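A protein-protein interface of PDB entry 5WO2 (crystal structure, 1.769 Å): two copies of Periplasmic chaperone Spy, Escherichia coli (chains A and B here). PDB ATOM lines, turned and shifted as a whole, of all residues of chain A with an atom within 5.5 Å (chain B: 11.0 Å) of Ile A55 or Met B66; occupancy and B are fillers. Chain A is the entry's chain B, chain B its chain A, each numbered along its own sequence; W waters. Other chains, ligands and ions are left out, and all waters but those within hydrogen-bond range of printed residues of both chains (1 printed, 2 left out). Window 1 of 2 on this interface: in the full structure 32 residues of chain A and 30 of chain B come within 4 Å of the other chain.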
ATOM      1  N   LYS A  50      16.936 -20.006  -6.481  1.00  0.00           N
ATOM      2  CA  LYS A  50      18.359 -19.995  -6.202  1.00  0.00           C
ATOM      3  C   LYS A  50      18.625 -20.041  -4.698  1.00  0.00           C
ATOM      4  O   LYS A  50      19.520 -20.730  -4.230  1.00  0.00           O
ATOM      5  CB  LYS A  50      18.976 -18.742  -6.831  1.00  0.00           C
ATOM      6  CG  LYS A  50      20.471 -18.821  -6.906  1.00  0.00           C
ATOM      7  CD  LYS A  50      21.035 -17.737  -7.838  1.00  0.00           C
ATOM      8  CE  LYS A  50      20.439 -17.773  -9.263  1.00  0.00           C
ATOM      9  NZ  LYS A  50      20.244 -19.159  -9.827  1.00  0.00           N
ATOM     10  N   ALA A  51      17.828 -19.311  -3.934  1.00  0.00           N
ATOM     11  CA  ALA A  51      17.996 -19.338  -2.483  1.00  0.00           C
ATOM     12  C   ALA A  51      17.698 -20.720  -1.945  1.00  0.00           C
ATOM     13  O   ALA A  51      18.401 -21.218  -1.058  1.00  0.00           O
ATOM     14  CB  ALA A  51      17.082 -18.270  -1.846  1.00  0.00           C
ATOM     15  N   GLU A  52      16.684 -21.365  -2.479  1.00  0.00           N
ATOM     16  CA  GLU A  52      16.377 -22.716  -2.029  1.00  0.00           C
ATOM     17  C   GLU A  52      17.548 -23.670  -2.302  1.00  0.00           C
ATOM     18  O   GLU A  52      17.838 -24.561  -1.490  1.00  0.00           O
ATOM     19  CB  GLU A  52      15.114 -23.238  -2.688  1.00  0.00           C
ATOM     20  CG  GLU A  52      13.859 -22.520  -2.177  1.00  0.00           C
ATOM     21  CD  GLU A  52      12.565 -22.985  -2.863  1.00  0.00           C
ATOM     22  OE1 GLU A  52      12.497 -22.992  -4.106  1.00  0.00           O
ATOM     23  OE2 GLU A  52      11.597 -23.276  -2.135  1.00  0.00           O
ATOM     24  N   ALA A  53      18.215 -23.498  -3.447  1.00  0.00           N
ATOM     25  CA  ALA A  53      19.340 -24.370  -3.734  1.00  0.00           C
ATOM     26  C   ALA A  53      20.501 -24.168  -2.752  1.00  0.00           C
ATOM     27  O   ALA A  53      21.136 -25.135  -2.307  1.00  0.00           O
ATOM     28  CB  ALA A  53      19.814 -24.174  -5.195  1.00  0.00           C
ATOM     29  N   GLN A  54      20.729 -22.919  -2.382  1.00  0.00           N
ATOM     30  CA  GLN A  54      21.767 -22.548  -1.402  1.00  0.00           C
ATOM     31  C   GLN A  54      21.446 -23.157  -0.066  1.00  0.00           C
ATOM     32  O   GLN A  54      22.321 -23.744   0.583  1.00  0.00           O
ATOM     33  CB  GLN A  54      21.885 -21.023  -1.258  1.00  0.00           C
ATOM     34  CG  GLN A  54      23.145 -20.584  -0.521  1.00  0.00           C
ATOM     35  CD  GLN A  54      23.003 -20.571   0.997  1.00  0.00           C
ATOM     36  OE1 GLN A  54      21.883 -20.574   1.530  1.00  0.00           O
ATOM     37  NE2 GLN A  54      24.149 -20.550   1.707  1.00  0.00           N
ATOM     38  N   ILE A  55      20.177 -23.092   0.326  1.00  0.00           N
ATOM     39  CA  ILE A  55      19.767 -23.666   1.601  1.00  0.00           C
ATOM     40  C   ILE A  55      19.971 -25.192   1.617  1.00  0.00           C
ATOM     41  O   ILE A  55      20.541 -25.768   2.559  1.00  0.00           O
ATOM     42  CB  ILE A  55      18.294 -23.305   1.921  1.00  0.00           C
ATOM     43  CG1 ILE A  55      18.163 -21.805   2.202  1.00  0.00           C
ATOM     44  CG2 ILE A  55      17.730 -24.172   3.100  1.00  0.00           C
ATOM     45  CD1 ILE A  55      16.744 -21.354   2.198  1.00  0.00           C
ATOM     46  N   ALA A  56      19.571 -25.862   0.545  1.00  0.00           N
ATOM     47  CA  ALA A  56      19.769 -27.302   0.426  1.00  0.00           C
ATOM     48  C   ALA A  56      21.248 -27.671   0.482  1.00  0.00           C
ATOM     49  O   ALA A  56      21.630 -28.683   1.094  1.00  0.00           O
ATOM     50  CB  ALA A  56      19.159 -27.774  -0.847  1.00  0.00           C
ATOM     51  N   LYS A  57      22.100 -26.879  -0.152  1.00  0.00           N
ATOM     52  CA  LYS A  57      23.520 -27.179  -0.106  1.00  0.00           C
ATOM     53  C   LYS A  57      24.055 -27.001   1.327  1.00  0.00           C
ATOM     54  O   LYS A  57      24.872 -27.809   1.814  1.00  0.00           O
ATOM     55  CB  LYS A  57      24.266 -26.314  -1.110  1.00  0.00           C
ATOM     56  CG  LYS A  57      25.774 -26.540  -1.119  1.00  0.00           C
ATOM     57  CD  LYS A  57      26.328 -26.692  -2.558  1.00  0.00           C
ATOM     58  CE  LYS A  57      27.649 -27.537  -2.601  1.00  0.00           C
ATOM     59  NZ  LYS A  57      27.481 -28.936  -2.082  1.00  0.00           N
ATOM     60  N   MET A  58      23.578 -25.972   2.016  1.00  0.00           N
ATOM     61  CA  MET A  58      24.004 -25.755   3.385  1.00  0.00           C
ATOM     62  C   MET A  58      23.570 -26.903   4.306  1.00  0.00           C
ATOM     63  O   MET A  58      24.268 -27.190   5.277  1.00  0.00           O
ATOM     64  CB  MET A  58      23.469 -24.438   3.894  1.00  0.00           C
ATOM     65  CG  MET A  58      24.088 -23.265   3.173  1.00  0.00           C
ATOM     66  SD  MET A  58      23.364 -21.728   3.741  1.00  0.00           S
ATOM     67  CE  MET A  58      24.029 -21.666   5.397  1.00  0.00           C
ATOM     68  N   GLU A  59      22.464 -27.594   3.986  1.00  0.00           N
ATOM     69  CA  GLU A  59      22.035 -28.761   4.775  1.00  0.00           C
ATOM     70  C   GLU A  59      23.114 -29.876   4.781  1.00  0.00           C
ATOM     71  O   GLU A  59      23.277 -30.597   5.791  1.00  0.00           O
ATOM     72  CB  GLU A  59      20.704 -29.338   4.270  1.00  0.00           C
ATOM     73  CG  GLU A  59      19.474 -28.499   4.545  1.00  0.00           C
ATOM     74  CD  GLU A  59      19.073 -28.456   6.033  1.00  0.00           C
ATOM     75  OE1 GLU A  59      19.183 -29.502   6.735  1.00  0.00           O
ATOM     76  OE2 GLU A  59      18.611 -27.391   6.481  1.00  0.00           O
ATOM     77  N   GLU B  33      13.978 -29.946  19.976  1.00  0.00           N
ATOM     78  CA  GLU B  33      15.185 -30.302  19.264  1.00  0.00           C
ATOM     79  C   GLU B  33      16.335 -30.542  20.217  1.00  0.00           C
ATOM     80  O   GLU B  33      17.125 -31.474  20.030  1.00  0.00           O
ATOM     81  CB  GLU B  33      15.565 -29.210  18.276  1.00  0.00           C
ATOM     82  CG  GLU B  33      16.488 -29.696  17.177  1.00  0.00           C
ATOM     83  CD  GLU B  33      15.732 -29.943  15.861  1.00  0.00           C
ATOM     84  OE1 GLU B  33      14.703 -30.660  15.892  1.00  0.00           O
ATOM     85  OE2 GLU B  33      16.157 -29.396  14.815  1.00  0.00           O
ATOM     86  N   ILE B  55      18.819 -34.734  12.942  1.00  0.00           N
ATOM     87  CA  ILE B  55      19.328 -33.570  12.235  1.00  0.00           C
ATOM     88  C   ILE B  55      18.361 -33.166  11.127  1.00  0.00           C
ATOM     89  O   ILE B  55      18.105 -31.988  10.907  1.00  0.00           O
ATOM     90  CB  ILE B  55      20.724 -33.881  11.675  1.00  0.00           C
ATOM     91  CG1 ILE B  55      21.701 -34.013  12.851  1.00  0.00           C
ATOM     92  CG2 ILE B  55      21.162 -32.879  10.649  1.00  0.00           C
ATOM     93  CD1 ILE B  55      22.997 -34.674  12.468  1.00  0.00           C
ATOM     94  N   ALA B  56      17.806 -34.164  10.428  1.00  0.00           N
ATOM     95  CA  ALA B  56      16.906 -33.885   9.320  1.00  0.00           C
ATOM     96  C   ALA B  56      15.498 -33.426   9.715  1.00  0.00           C
ATOM     97  O   ALA B  56      14.799 -32.841   8.855  1.00  0.00           O
ATOM     98  CB  ALA B  56      16.788 -35.098   8.426  1.00  0.00           C
ATOM     99  N   MET B  58      13.765 -31.018  11.376  1.00  0.00           N
ATOM    100  CA  MET B  58      13.222 -29.671  11.127  1.00  0.00           C
ATOM    101  C   MET B  58      13.818 -29.014   9.876  1.00  0.00           C
ATOM    102  O   MET B  58      14.011 -27.801   9.825  1.00  0.00           O
ATOM    103  CB  MET B  58      13.440 -28.776  12.356  1.00  0.00           C
ATOM    104  CG  MET B  58      12.603 -29.201  13.584  1.00  0.00           C
ATOM    105  SD  MET B  58      12.647 -28.076  15.012  1.00  0.00           S
ATOM    106  CE  MET B  58      12.092 -26.569  14.240  1.00  0.00           C
ATOM    107  N   GLU B  59      14.097 -29.822   8.858  1.00  0.00           N
ATOM    108  CA  GLU B  59      14.507 -29.319   7.537  1.00  0.00           C
ATOM    109  C   GLU B  59      13.561 -28.285   6.924  1.00  0.00           C
ATOM    110  O   GLU B  59      13.998 -27.241   6.420  1.00  0.00           O
ATOM    111  CB  GLU B  59      14.640 -30.517   6.578  1.00  0.00           C
ATOM    112  CG  GLU B  59      15.050 -30.160   5.177  1.00  0.00           C
ATOM    113  CD  GLU B  59      15.007 -31.395   4.245  1.00  0.00           C
ATOM    114  OE1 GLU B  59      15.511 -32.409   4.695  1.00  0.00           O
ATOM    115  OE2 GLU B  59      14.508 -31.313   3.095  1.00  0.00           O
ATOM    116  N   GLU B  60      12.264 -28.587   6.945  1.00  0.00           N
ATOM    117  CA  GLU B  60      11.250 -27.660   6.402  1.00  0.00           C
ATOM    118  C   GLU B  60      11.181 -26.339   7.140  1.00  0.00           C
ATOM    119  O   GLU B  60      11.074 -25.267   6.520  1.00  0.00           O
ATOM    120  CB  GLU B  60       9.868 -28.312   6.430  1.00  0.00           C
ATOM    121  CG  GLU B  60       9.660 -29.333   5.323  1.00  0.00           C
ATOM    122  CD  GLU B  60      10.032 -28.758   3.973  1.00  0.00           C
ATOM    123  OE1 GLU B  60       9.303 -27.857   3.475  1.00  0.00           O
ATOM    124  OE2 GLU B  60      11.093 -29.160   3.451  1.00  0.00           O
ATOM    125  N   GLN B  61      11.228 -26.403   8.464  1.00  0.00           N
ATOM    126  CA  GLN B  61      11.150 -25.171   9.264  1.00  0.00           C
ATOM    127  C   GLN B  61      12.406 -24.316   9.054  1.00  0.00           C
ATOM    128  O   GLN B  61      12.334 -23.092   8.975  1.00  0.00           O
ATOM    129  CB  GLN B  61      10.943 -25.530  10.738  1.00  0.00           C
ATOM    130  CG  GLN B  61       9.578 -26.255  11.045  1.00  0.00           C
ATOM    131  CD  GLN B  61       9.552 -27.809  10.906  1.00  0.00           C
ATOM    132  OE1 GLN B  61      10.110 -28.408   9.971  1.00  0.00           O
ATOM    133  NE2 GLN B  61       8.878 -28.459  11.860  1.00  0.00           N
ATOM    134  N   ARG B  62      13.556 -24.973   8.952  1.00  0.00           N
ATOM    135  CA  ARG B  62      14.815 -24.301   8.656  1.00  0.00           C
ATOM    136  C   ARG B  62      14.754 -23.621   7.307  1.00  0.00           C
ATOM    137  O   ARG B  62      15.199 -22.467   7.162  1.00  0.00           O
ATOM    138  CB  ARG B  62      15.975 -25.313   8.676  1.00  0.00           C
ATOM    139  CG  ARG B  62      16.419 -25.668  10.064  1.00  0.00           C
ATOM    140  CD  ARG B  62      17.777 -26.330  10.046  1.00  0.00           C
ATOM    141  NE  ARG B  62      17.780 -27.583   9.298  1.00  0.00           N
ATOM    142  CZ  ARG B  62      17.502 -28.776   9.834  1.00  0.00           C
ATOM    143  NH1 ARG B  62      17.151 -28.896  11.102  1.00  0.00           N
ATOM    144  NH2 ARG B  62      17.561 -29.829   9.072  1.00  0.00           N
ATOM    145  N   LYS B  63      14.215 -24.332   6.320  1.00  0.00           N
ATOM    146  CA  LYS B  63      14.087 -23.764   4.969  1.00  0.00           C
ATOM    147  C   LYS B  63      13.227 -22.491   5.008  1.00  0.00           C
ATOM    148  O   LYS B  63      13.617 -21.450   4.471  1.00  0.00           O
ATOM    149  CB  LYS B  63      13.476 -24.761   4.005  1.00  0.00           C
ATOM    150  CG  LYS B  63      13.286 -24.234   2.587  1.00  0.00           C
ATOM    151  CD  LYS B  63      12.590 -25.238   1.720  1.00  0.00           C
ATOM    152  CE  LYS B  63      12.366 -24.748   0.284  1.00  0.00           C
ATOM    153  NZ  LYS B  63      11.767 -25.868  -0.470  1.00  0.00           N
ATOM    154  N   ALA B  64      12.063 -22.576   5.632  1.00  0.00           N
ATOM    155  CA  ALA B  64      11.166 -21.405   5.713  1.00  0.00           C
ATOM    156  C   ALA B  64      11.879 -20.267   6.400  1.00  0.00           C
ATOM    157  O   ALA B  64      11.771 -19.119   6.009  1.00  0.00           O
ATOM    158  CB  ALA B  64       9.854 -21.765   6.462  1.00  0.00           C
ATOM    159  N   ASN B  65      12.617 -20.582   7.459  1.00  0.00           N
ATOM    160  CA  ASN B  65      13.256 -19.516   8.229  1.00  0.00           C
ATOM    161  C   ASN B  65      14.371 -18.871   7.452  1.00  0.00           C
ATOM    162  O   ASN B  65      14.524 -17.654   7.436  1.00  0.00           O
ATOM    163  CB  ASN B  65      13.799 -20.054   9.548  1.00  0.00           C
ATOM    164  CG  ASN B  65      12.712 -20.332  10.546  1.00  0.00           C
ATOM    165  OD1 ASN B  65      11.606 -19.797  10.454  1.00  0.00           O
ATOM    166  ND2 ASN B  65      13.023 -21.158  11.524  1.00  0.00           N
ATOM    167  N   MET B  66      15.152 -19.676   6.751  1.00  0.00           N
ATOM    168  CA  MET B  66      16.318 -19.138   6.054  1.00  0.00           C
ATOM    169  C   MET B  66      15.923 -18.426   4.755  1.00  0.00           C
ATOM    170  O   MET B  66      16.609 -17.510   4.284  1.00  0.00           O
ATOM    171  CB  MET B  66      17.307 -20.268   5.776  1.00  0.00           C
ATOM    172  CG  MET B  66      17.880 -20.806   7.091  1.00  0.00           C
ATOM    173  SD  MET B  66      18.484 -22.500   6.896  1.00  0.00           S
ATOM    174  CE  MET B  66      19.141 -22.786   8.551  1.00  0.00           C
ATOM    175  N   LEU B  67      14.806 -18.823   4.184  1.00  0.00           N
ATOM    176  CA  LEU B  67      14.286 -18.080   3.034  1.00  0.00           C
ATOM    177  C   LEU B  67      13.792 -16.732   3.452  1.00  0.00           C
ATOM    178  O   LEU B  67      14.034 -15.713   2.772  1.00  0.00           O
ATOM    179  CB  LEU B  67      13.150 -18.818   2.372  1.00  0.00           C
ATOM    180  CG  LEU B  67      13.521 -19.937   1.404  1.00  0.00           C
ATOM    181  CD1 LEU B  67      12.277 -20.688   0.984  1.00  0.00           C
ATOM    182  CD2 LEU B  67      14.190 -19.318   0.194  1.00  0.00           C
ATOM    183  N   ALA B  68      13.075 -16.698   4.565  1.00  0.00           N
ATOM    184  CA  ALA B  68      12.627 -15.402   5.127  1.00  0.00           C
ATOM    185  C   ALA B  68      13.804 -14.489   5.431  1.00  0.00           C
ATOM    186  O   ALA B  68      13.792 -13.273   5.118  1.00  0.00           O
ATOM    187  CB  ALA B  68      11.835 -15.639   6.367  1.00  0.00           C
ATOM    188  N   HIS B  69      14.840 -15.059   6.041  1.00  0.00           N
ATOM    189  CA  HIS B  69      16.010 -14.274   6.416  1.00  0.00           C
ATOM    190  C   HIS B  69      16.685 -13.728   5.169  1.00  0.00           C
ATOM    191  O   HIS B  69      16.958 -12.523   5.087  1.00  0.00           O
ATOM    192  CB  HIS B  69      16.995 -15.120   7.264  1.00  0.00           C
ATOM    193  CG  HIS B  69      18.259 -14.400   7.657  1.00  0.00           C
ATOM    194  ND1 HIS B  69      18.316 -13.460   8.670  1.00  0.00           N
ATOM    195  CD2 HIS B  69      19.521 -14.496   7.168  1.00  0.00           C
ATOM    196  CE1 HIS B  69      19.550 -13.002   8.781  1.00  0.00           C
ATOM    197  NE2 HIS B  69      20.302 -13.613   7.881  1.00  0.00           N
ATOM    198  N   MET B  70      16.895 -14.571   4.172  1.00  0.00           N
ATOM    199  CA  MET B  70      17.663 -14.154   3.004  1.00  0.00           C
ATOM    200  C   MET B  70      16.837 -13.115   2.230  1.00  0.00           C
ATOM    201  O   MET B  70      17.389 -12.120   1.723  1.00  0.00           O
ATOM    202  CB  MET B  70      18.052 -15.338   2.122  1.00  0.00           C
ATOM    203  CG  MET B  70      18.999 -16.265   2.796  1.00  0.00           C
ATOM    204  SD  MET B  70      19.112 -17.809   1.820  1.00  0.00           S
ATOM    205  CE  MET B  70      20.315 -17.060   0.809  1.00  0.00           C
ATOM    206  N   GLU B  71      15.520 -13.275   2.209  1.00  0.00           N
ATOM    207  CA  GLU B  71      14.729 -12.326   1.431  1.00  0.00           C
ATOM    208  C   GLU B  71      14.744 -10.983   2.119  1.00  0.00           C
ATOM    209  O   GLU B  71      14.854  -9.932   1.462  1.00  0.00           O
ATOM    210  CB  GLU B  71      13.302 -12.807   1.244  1.00  0.00           C
ATOM    211  CG  GLU B  71      12.515 -11.834   0.323  1.00  0.00           C
ATOM    212  CD  GLU B  71      11.210 -12.382  -0.203  1.00  0.00           C
ATOM    213  OE1 GLU B  71      10.772 -13.418   0.294  1.00  0.00           O
ATOM    214  OE2 GLU B  71      10.595 -11.752  -1.115  1.00  0.00           O
ATOM    215  N   THR B  72      14.596 -11.007   3.442  1.00  0.00           N
ATOM    216  CA  THR B  72      14.657  -9.777   4.206  1.00  0.00           C
ATOM    217  C   THR B  72      15.982  -9.077   4.024  1.00  0.00           C
ATOM    218  O   THR B  72      16.026  -7.861   3.804  1.00  0.00           O
ATOM    219  CB  THR B  72      14.421 -10.057   5.676  1.00  0.00           C
ATOM    220  OG1 THR B  72      13.071 -10.521   5.822  1.00  0.00           O
ATOM    221  CG2 THR B  72      14.621  -8.800   6.552  1.00  0.00           C
ATOM    222  N   GLN B  73      17.067  -9.817   4.101  1.00  0.00           N
ATOM    223  CA  GLN B  73      18.390  -9.199   3.935  1.00  0.00           C
ATOM    224  C   GLN B  73      18.571  -8.620   2.537  1.00  0.00           C
ATOM    225  O   GLN B  73      19.173  -7.552   2.389  1.00  0.00           O
ATOM    226  CB  GLN B  73      19.490 -10.194   4.222  1.00  0.00           C
ATOM    227  CG  GLN B  73      19.542 -10.648   5.665  1.00  0.00           C
ATOM    228  CD  GLN B  73      20.051  -9.560   6.617  1.00  0.00           C
ATOM    229  OE1 GLN B  73      21.055  -8.912   6.331  1.00  0.00           O
ATOM    230  NE2 GLN B  73      19.354  -9.346   7.748  1.00  0.00           N
ATOM    231  N   ASN B  74      18.030  -9.297   1.520  1.00  0.00           N
ATOM    232  CA  ASN B  74      18.080  -8.775   0.168  1.00  0.00           C
ATOM    233  C   ASN B  74      17.272  -7.499   0.053  1.00  0.00           C
ATOM    234  O   ASN B  74      17.696  -6.545  -0.621  1.00  0.00           O
ATOM    235  CB  ASN B  74      17.571  -9.819  -0.831  1.00  0.00           C
ATOM    236  CG  ASN B  74      17.510  -9.284  -2.252  1.00  0.00           C
ATOM    237  OD1 ASN B  74      16.514  -8.720  -2.664  1.00  0.00           O
ATOM    238  ND2 ASN B  74      18.554  -9.518  -3.013  1.00  0.00           N
ATOM    239  N   LYS B  75      16.105  -7.456   0.681  1.00  0.00           N
ATOM    240  CA  LYS B  75      15.291  -6.223   0.599  1.00  0.00           C
ATOM    241  C   LYS B  75      16.043  -5.049   1.235  1.00  0.00           C
ATOM    242  O   LYS B  75      16.038  -3.929   0.720  1.00  0.00           O
ATOM    243  CB  LYS B  75      13.952  -6.424   1.279  1.00  0.00           C
ATOM    244  CG  LYS B  75      12.970  -7.273   0.445  1.00  0.00           C
ATOM    245  CD  LYS B  75      11.645  -7.406   1.186  1.00  0.00           C
ATOM    246  CE  LYS B  75      10.655  -8.271   0.448  1.00  0.00           C
ATOM    247  NZ  LYS B  75       9.480  -8.495   1.334  1.00  0.00           N
HETATM  248  O   HOH W   1      16.356 -26.688   5.065  1.00  0.00           O
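The side-chain carboxylate (OE1) of Glu A59 is in salt-bridge range of the guanidinium group (NH2) of Arg B62. The side-chain carboxylate of Glu A52 is in salt-bridge range of the side-chain amino group of Lys B63 (3.1 Å).
The side-chain amide nitrogen (NE2) of Gln A54 lies within hydrogen-bond range of the side-chain sulfur (SD) of Met A58 (2.5 Å). The side-chain carboxylate of Glu B33 lies within salt-bridge range of the guanidinium group of Arg B62 (3.9 Å). The backbone carbonyl oxygen (O) of Ile B55 lies within hydrogen-bond range of the guanidinium group (NH2) of Arg B62, 2.9 Å away.
Among the printed residues, merely in contact across the chains: Ala A51 with Leu B67 (3.7 Å), Glu A52 with Leu B67 (3.98 Å), Gln A54 with Met B70 (3.9 Å), Ile A55 with Lys B63 (3.9 Å), Ile A55 with Met B66 (3.8 Å) and Ile A55 with Leu B67 (3.6 Å).
Of the printed residues of chain B, Ile A55 touches Lys B63 (3.9 Å), Met B66 (3.8 Å) and Leu B67 (3.6 Å). Ala A51 touches just one residue of chain B: Leu B67 (3.7 Å). No residue of chain B comes within 4 Å of Ala A53. Gln A54 touches just one residue of chain B: Met B70 (3.9 Å). Of chain B, only Arg B62 (2.9 Å) comes within 4 Å of Glu A59. Printed residues of chain A within 4 Å of Met B70: Gln A54 (3.9 Å). Of the printed residues of chain A, Leu B67 touches Ala A51 (3.7 Å), Glu A52 (3.98 Å) and Ile A55 (3.6 Å). Glu B59 touches none of the printed residues of chain A. Gln B61 touches none of the printed residues of chain A. The nearest printed residue of chain A that does not touch Met B70 is Ile A55 (4.1 Å).
Of the 10 printed residues of chain A, 5 touch a printed residue of chain B. Hydrophobic or aromatic side chains of chain A that line the printed part of chain B: Ala A51 and Ile A55. Among the printed residues, 8 pairs touch across the chains.
4 positions are printed for both chains.
Water W1 lies within hydrogen-bond range of the side-chain carboxylate of Glu A59 (2.8 Å), the backbone carbonyl oxygen of Glu B59 (2.8 Å) and the backbone NH of Lys B63 (3.4 Å).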
